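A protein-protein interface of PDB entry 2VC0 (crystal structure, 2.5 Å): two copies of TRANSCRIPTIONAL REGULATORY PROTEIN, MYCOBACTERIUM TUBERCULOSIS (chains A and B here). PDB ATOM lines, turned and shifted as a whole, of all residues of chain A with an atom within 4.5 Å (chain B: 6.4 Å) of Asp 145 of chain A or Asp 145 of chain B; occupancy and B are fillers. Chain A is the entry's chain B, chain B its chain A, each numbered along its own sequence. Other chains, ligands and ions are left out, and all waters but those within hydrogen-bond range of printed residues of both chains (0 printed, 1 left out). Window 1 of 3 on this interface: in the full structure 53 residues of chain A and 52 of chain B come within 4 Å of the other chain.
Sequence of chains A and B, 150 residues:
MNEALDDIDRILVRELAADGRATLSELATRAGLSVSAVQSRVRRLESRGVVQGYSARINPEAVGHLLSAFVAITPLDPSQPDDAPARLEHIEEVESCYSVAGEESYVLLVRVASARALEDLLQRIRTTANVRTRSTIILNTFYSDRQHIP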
ATOM      1  N   ARG A  57      11.862 -19.580  -0.275  1.00  0.00           N
ATOM      2  CA  ARG A  57      11.515 -19.272  -1.633  1.00  0.00           C
ATOM      3  C   ARG A  57      10.007 -19.150  -1.847  1.00  0.00           C
ATOM      4  O   ARG A  57       9.247 -20.121  -1.950  1.00  0.00           O
ATOM      5  CB  ARG A  57      12.229 -20.224  -2.562  1.00  0.00           C
ATOM      6  CG  ARG A  57      13.760 -19.779  -2.647  1.00  0.00           C
ATOM      7  CD  ARG A  57      14.487 -20.430  -3.832  1.00  0.00           C
ATOM      8  NE  ARG A  57      13.964 -21.800  -4.000  1.00  0.00           N
ATOM      9  CZ  ARG A  57      14.494 -22.894  -3.437  1.00  0.00           C
ATOM     10  NH1 ARG A  57      15.625 -22.799  -2.718  1.00  0.00           N
ATOM     11  NH2 ARG A  57      13.920 -24.087  -3.619  1.00  0.00           N
ATOM     12  N   GLU A  95      13.532  -6.309  -6.902  1.00  0.00           N
ATOM     13  CA  GLU A  95      14.135  -7.407  -6.309  1.00  0.00           C
ATOM     14  C   GLU A  95      15.642  -7.538  -6.605  1.00  0.00           C
ATOM     15  O   GLU A  95      16.371  -8.069  -5.763  1.00  0.00           O
ATOM     16  CB  GLU A  95      13.435  -8.583  -6.922  1.00  0.00           C
ATOM     17  CG  GLU A  95      13.825  -9.856  -6.347  1.00  0.00           C
ATOM     18  CD  GLU A  95      12.810 -10.914  -6.602  1.00  0.00           C
ATOM     19  OE1 GLU A  95      13.310 -11.996  -6.911  1.00  0.00           O
ATOM     20  OE2 GLU A  95      11.562 -10.686  -6.481  1.00  0.00           O
ATOM     21  N   SER A  96      16.126  -7.126  -7.776  1.00  0.00           N
ATOM     22  CA  SER A  96      17.548  -7.318  -8.103  1.00  0.00           C
ATOM     23  C   SER A  96      18.081  -6.247  -8.961  1.00  0.00           C
ATOM     24  O   SER A  96      17.370  -5.652  -9.808  1.00  0.00           O
ATOM     25  CB  SER A  96      17.747  -8.607  -8.800  1.00  0.00           C
ATOM     26  OG  SER A  96      17.659  -9.647  -7.846  1.00  0.00           O
ATOM     27  N   SER A 144      14.577 -21.409 -10.921  1.00  0.00           N
ATOM     28  CA  SER A 144      15.061 -20.169 -10.460  1.00  0.00           C
ATOM     29  C   SER A 144      16.074 -20.569  -9.367  1.00  0.00           C
ATOM     30  O   SER A 144      16.028 -21.653  -8.879  1.00  0.00           O
ATOM     31  CB  SER A 144      13.833 -19.436  -9.948  1.00  0.00           C
ATOM     32  OG  SER A 144      14.156 -18.399  -9.053  1.00  0.00           O
ATOM     33  N   ASP A 145      16.981 -19.692  -8.979  1.00  0.00           N
ATOM     34  CA  ASP A 145      18.209 -20.043  -8.217  1.00  0.00           C
ATOM     35  C   ASP A 145      18.476 -21.443  -7.770  1.00  0.00           C
ATOM     36  O   ASP A 145      18.436 -21.713  -6.609  1.00  0.00           O
ATOM     37  CB  ASP A 145      18.432 -19.114  -7.009  1.00  0.00           C
ATOM     38  CG  ASP A 145      17.152 -18.496  -6.538  1.00  0.00           C
ATOM     39  OD1 ASP A 145      17.031 -17.256  -6.732  1.00  0.00           O
ATOM     40  OD2 ASP A 145      16.280 -19.265  -6.057  1.00  0.00           O
ATOM     41  N   ARG A 146      18.784 -22.324  -8.701  1.00  0.00           N
ATOM     42  CA  ARG A 146      19.361 -23.542  -8.353  1.00  0.00           C
ATOM     43  C   ARG A 146      20.840 -23.358  -8.412  1.00  0.00           C
ATOM     44  O   ARG A 146      21.437 -23.468  -9.465  1.00  0.00           O
ATOM     45  CB  ARG A 146      18.847 -24.655  -9.224  1.00  0.00           C
ATOM     46  CG  ARG A 146      19.279 -24.796 -10.597  1.00  0.00           C
ATOM     47  CD  ARG A 146      18.186 -25.588 -11.191  1.00  0.00           C
ATOM     48  NE  ARG A 146      18.470 -26.497 -12.311  1.00  0.00           N
ATOM     49  CZ  ARG A 146      19.490 -26.493 -13.152  1.00  0.00           C
ATOM     50  NH1 ARG A 146      20.482 -25.634 -13.098  1.00  0.00           N
ATOM     51  NH2 ARG A 146      19.517 -27.417 -14.068  1.00  0.00           N
ATOM     52  N   GLN A 147      21.388 -22.996  -7.250  1.00  0.00           N
ATOM     53  CA  GLN A 147      22.807 -22.781  -6.989  1.00  0.00           C
ATOM     54  C   GLN A 147      23.656 -24.040  -7.165  1.00  0.00           C
ATOM     55  O   GLN A 147      23.317 -25.100  -6.688  1.00  0.00           O
ATOM     56  CB  GLN A 147      23.012 -22.215  -5.569  1.00  0.00           C
ATOM     57  CG  GLN A 147      22.299 -20.888  -5.317  1.00  0.00           C
ATOM     58  CD  GLN A 147      22.206 -20.508  -3.823  1.00  0.00           C
ATOM     59  OE1 GLN A 147      22.873 -19.541  -3.346  1.00  0.00           O
ATOM     60  NE2 GLN A 147      21.350 -21.237  -3.086  1.00  0.00           N
ATOM     61  N   SER B  55      16.590 -22.145   1.360  1.00  0.00           N
ATOM     62  CA  SER B  55      17.919 -22.203   0.767  1.00  0.00           C
ATOM     63  C   SER B  55      18.827 -21.283   1.482  1.00  0.00           C
ATOM     64  O   SER B  55      18.432 -20.157   1.882  1.00  0.00           O
ATOM     65  CB  SER B  55      17.891 -21.783  -0.756  1.00  0.00           C
ATOM     66  N   ARG B  57      21.533 -18.624   1.019  1.00  0.00           N
ATOM     67  CA  ARG B  57      22.011 -17.713   0.002  1.00  0.00           C
ATOM     68  C   ARG B  57      23.559 -17.776   0.044  1.00  0.00           C
ATOM     69  O   ARG B  57      24.204 -17.178   0.923  1.00  0.00           O
ATOM     70  CB  ARG B  57      21.491 -16.296   0.281  1.00  0.00           C
ATOM     71  N   GLU B  95      21.582 -21.528 -13.644  1.00  0.00           N
ATOM     72  CA  GLU B  95      20.903 -21.403 -12.389  1.00  0.00           C
ATOM     73  C   GLU B  95      19.466 -20.964 -12.519  1.00  0.00           C
ATOM     74  O   GLU B  95      18.711 -21.175 -11.594  1.00  0.00           O
ATOM     75  CB  GLU B  95      21.651 -20.381 -11.549  1.00  0.00           C
ATOM     76  CG  GLU B  95      20.887 -19.791 -10.333  1.00  0.00           C
ATOM     77  CD  GLU B  95      21.850 -18.851  -9.512  1.00  0.00           C
ATOM     78  OE1 GLU B  95      21.377 -17.831  -8.880  1.00  0.00           O
ATOM     79  OE2 GLU B  95      23.093 -19.157  -9.581  1.00  0.00           O
ATOM     80  N   SER B  96      19.067 -20.292 -13.601  1.00  0.00           N
ATOM     81  CA  SER B  96      17.657 -19.859 -13.755  1.00  0.00           C
ATOM     82  C   SER B  96      17.316 -19.885 -15.228  1.00  0.00           C
ATOM     83  O   SER B  96      18.185 -19.669 -16.096  1.00  0.00           O
ATOM     84  CB  SER B  96      17.481 -18.418 -13.315  1.00  0.00           C
ATOM     85  OG  SER B  96      17.778 -18.203 -11.963  1.00  0.00           O
ATOM     86  N   TYR B  98      14.036 -18.536 -17.772  1.00  0.00           N
ATOM     87  CA  TYR B  98      12.740 -17.840 -17.859  1.00  0.00           C
ATOM     88  C   TYR B  98      12.305 -17.768 -19.294  1.00  0.00           C
ATOM     89  O   TYR B  98      13.140 -17.554 -20.201  1.00  0.00           O
ATOM     90  CB  TYR B  98      12.920 -16.394 -17.466  1.00  0.00           C
ATOM     91  CG  TYR B  98      13.461 -16.172 -16.120  1.00  0.00           C
ATOM     92  CD1 TYR B  98      14.828 -15.948 -15.921  1.00  0.00           C
ATOM     93  CD2 TYR B  98      12.596 -16.131 -15.001  1.00  0.00           C
ATOM     94  CE1 TYR B  98      15.363 -15.691 -14.570  1.00  0.00           C
ATOM     95  CE2 TYR B  98      13.087 -15.891 -13.694  1.00  0.00           C
ATOM     96  CZ  TYR B  98      14.454 -15.725 -13.490  1.00  0.00           C
ATOM     97  OH  TYR B  98      14.882 -15.504 -12.225  1.00  0.00           O
ATOM     98  N   TYR B 143      22.426  -6.044  -5.371  1.00  0.00           N
ATOM     99  CA  TYR B 143      21.552  -6.697  -4.385  1.00  0.00           C
ATOM    100  C   TYR B 143      20.662  -7.653  -5.164  1.00  0.00           C
ATOM    101  O   TYR B 143      20.317  -7.375  -6.351  1.00  0.00           O
ATOM    102  CB  TYR B 143      20.723  -5.705  -3.516  1.00  0.00           C
ATOM    103  CG  TYR B 143      20.206  -4.472  -4.214  1.00  0.00           C
ATOM    104  CD1 TYR B 143      20.986  -3.316  -4.264  1.00  0.00           C
ATOM    105  CD2 TYR B 143      18.907  -4.426  -4.822  1.00  0.00           C
ATOM    106  CE1 TYR B 143      20.512  -2.107  -4.916  1.00  0.00           C
ATOM    107  CE2 TYR B 143      18.415  -3.211  -5.490  1.00  0.00           C
ATOM    108  CZ  TYR B 143      19.240  -2.087  -5.549  1.00  0.00           C
ATOM    109  OH  TYR B 143      18.867  -0.882  -6.162  1.00  0.00           O
ATOM    110  N   SER B 144      20.274  -8.744  -4.537  1.00  0.00           N
ATOM    111  CA  SER B 144      19.384  -9.627  -5.233  1.00  0.00           C
ATOM    112  C   SER B 144      18.426 -10.388  -4.331  1.00  0.00           C
ATOM    113  O   SER B 144      18.618 -10.489  -3.128  1.00  0.00           O
ATOM    114  CB  SER B 144      20.173 -10.628  -6.023  1.00  0.00           C
ATOM    115  OG  SER B 144      21.290 -10.961  -5.252  1.00  0.00           O
ATOM    116  N   ASP B 145      17.406 -10.950  -4.937  1.00  0.00           N
ATOM    117  CA  ASP B 145      16.439 -11.716  -4.189  1.00  0.00           C
ATOM    118  C   ASP B 145      15.891 -10.916  -3.069  1.00  0.00           C
ATOM    119  O   ASP B 145      15.658 -11.403  -2.036  1.00  0.00           O
ATOM    120  CB  ASP B 145      17.037 -12.992  -3.601  1.00  0.00           C
ATOM    121  CG  ASP B 145      17.915 -13.666  -4.560  1.00  0.00           C
ATOM    122  OD1 ASP B 145      17.424 -14.453  -5.420  1.00  0.00           O
ATOM    123  OD2 ASP B 145      19.117 -13.324  -4.501  1.00  0.00           O
ATOM    124  N   ARG B 146      15.648  -9.674  -3.258  1.00  0.00           N
ATOM    125  CA  ARG B 146      15.163  -9.007  -2.160  1.00  0.00           C
ATOM    126  C   ARG B 146      13.631  -9.168  -2.272  1.00  0.00           C
ATOM    127  O   ARG B 146      12.975  -8.426  -2.921  1.00  0.00           O
ATOM    128  CB  ARG B 146      15.918  -7.720  -2.268  1.00  0.00           C
ATOM    129  CG  ARG B 146      15.386  -6.499  -2.023  1.00  0.00           C
ATOM    130  CD  ARG B 146      16.451  -5.733  -2.597  1.00  0.00           C
ATOM    131  NE  ARG B 146      16.590  -4.482  -2.187  1.00  0.00           N
ATOM    132  CZ  ARG B 146      16.237  -3.439  -2.907  1.00  0.00           C
ATOM    133  NH1 ARG B 146      15.677  -3.542  -4.094  1.00  0.00           N
ATOM    134  NH2 ARG B 146      16.458  -2.237  -2.393  1.00  0.00           N
ATOM    135  N   GLN B 147      13.093 -10.275  -1.722  1.00  0.00           N
ATOM    136  CA  GLN B 147      11.696 -10.714  -1.949  1.00  0.00           C
ATOM    137  C   GLN B 147      10.799  -9.822  -1.183  1.00  0.00           C
ATOM    138  O   GLN B 147      11.104  -9.526  -0.038  1.00  0.00           O
ATOM    139  CB  GLN B 147      11.405 -12.186  -1.530  1.00  0.00           C
ATOM    140  CG  GLN B 147      12.360 -13.208  -2.079  1.00  0.00           C
ATOM    141  CD  GLN B 147      12.018 -14.628  -1.691  1.00  0.00           C
ATOM    142  OE1 GLN B 147      11.064 -15.185  -2.222  1.00  0.00           O
ATOM    143  NE2 GLN B 147      12.826 -15.244  -0.821  1.00  0.00           N
ATOM    144  N   HIS B 148       9.694  -9.393  -1.801  1.00  0.00           N
ATOM    145  CA  HIS B 148       8.787  -8.367  -1.272  1.00  0.00           C
ATOM    146  C   HIS B 148       7.368  -8.939  -1.111  1.00  0.00           C
ATOM    147  O   HIS B 148       6.737  -9.428  -2.073  1.00  0.00           O
ATOM    148  CB  HIS B 148       8.823  -7.173  -2.188  1.00  0.00           C
ATOM    149  CG  HIS B 148       7.724  -6.166  -1.962  1.00  0.00           C
ATOM    150  ND1 HIS B 148       7.513  -5.529  -0.745  1.00  0.00           N
ATOM    151  CD2 HIS B 148       6.804  -5.648  -2.822  1.00  0.00           C
ATOM    152  CE1 HIS B 148       6.504  -4.679  -0.867  1.00  0.00           C
ATOM    153  NE2 HIS B 148       6.062  -4.730  -2.117  1.00  0.00           N
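N of Asp 145 of chain A is in hydrogen-bond range of O of Glu 95 of chain B (3.5 Å).
The backbone NH (N) of Arg 146 of chain A lies within hydrogen-bond range of the backbone carbonyl oxygen (O) of Glu 95 of chain B.
The backbone NH (N) of Asp 145 of chain A lies within hydrogen-bond range of the side-chain hydroxyl (OG) of Ser 96 of chain B (3.4 Å).
The backbone NH (N) of Asp 145 of chain B is in hydrogen-bond range of the backbone carbonyl oxygen (O) of Glu 95 of chain A, 3.2 Å away.
N of Asp 145 of chain B is in hydrogen-bond range of OG of Ser 96 of chain A.
The backbone NH (N) of Arg 146 of chain B lies within hydrogen-bond range of the backbone carbonyl oxygen (O) of Glu 95 of chain A (3.1 Å).
The side-chain carboxylate of Asp 145 of chain A sits close to the side-chain carboxylate of Asp 145 of chain B, 3.1 Å away.
OG of Ser 144 of chain B lies close to OD2 of Asp 145 of chain B (3.3 Å).
Among the printed residues, pairs that only touch across the chains: Arg 57 of chain A with Ser 55 of chain B, Glu 95 of chain A with Ser 144 of chain B, Ser 96 of chain A with Tyr 143 of chain B, Ser 96 of chain A with Ser 144 of chain B, Ser 144 of chain A with Glu 95 of chain B, Ser 144 of chain A with Ser 96 of chain B and Gln 147 of chain A with Arg 57 of chain B.
Of the printed residues of chain B, Ser 144 of chain A touches Glu 95 and Ser 96.
Of the printed residues of chain A, Arg 57 of chain B touches Gln 147.
Printed residues of chain A within 4 Å of Ser 96 of chain B: Ser 144 and Asp 145.
Of chain A, only Glu 95, Ser 96 and Asp 145 come within 4 Å of Asp 145 of chain B.
Gln 147 of chain B touches none of the printed residues of chain A.
His 148 of chain B touches none of the printed residues of chain A.
The nearest residue of chain B that does not touch Asp 145 of chain A is Tyr 98 of chain B (5.7 Å).
The nearest printed residue of chain A that does not touch Asp 145 of chain B is Ser 144 of chain A (6.3 Å).
The nearest printed residue of chain A that does not touch Tyr 143 of chain B is Glu 95 of chain A (4.05 Å).
Among the printed residues, 14 pairs touch across the chains.
Among the printed residues, no Asp or Glu carboxylate lies within 4 Å of a Lys or Arg side-chain nitrogen of the other chain.
Glu 95 of chain A touches Ser 144 of chain B, and with the chains exchanged Ser 144 of chain A touches Glu 95 of chain B.
Ser 96 of chain A touches Ser 144 of chain B, and with the chains exchanged Ser 144 of chain A touches Ser 96 of chain B.
Ser 96 of chain A touches Asp 145 of chain B, and with the chains exchanged Asp 145 of chain A touches Ser 96 of chain B.
Gln 147 of chain A touches Arg 57 of chain B, but with the chains exchanged Arg 57 of chain A does not touch Gln 147 of chain B (4.1 Å).
Of the 14 pairs that touch across the chains among the printed residues, 11 have their exchanged pair printed and touching as well.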
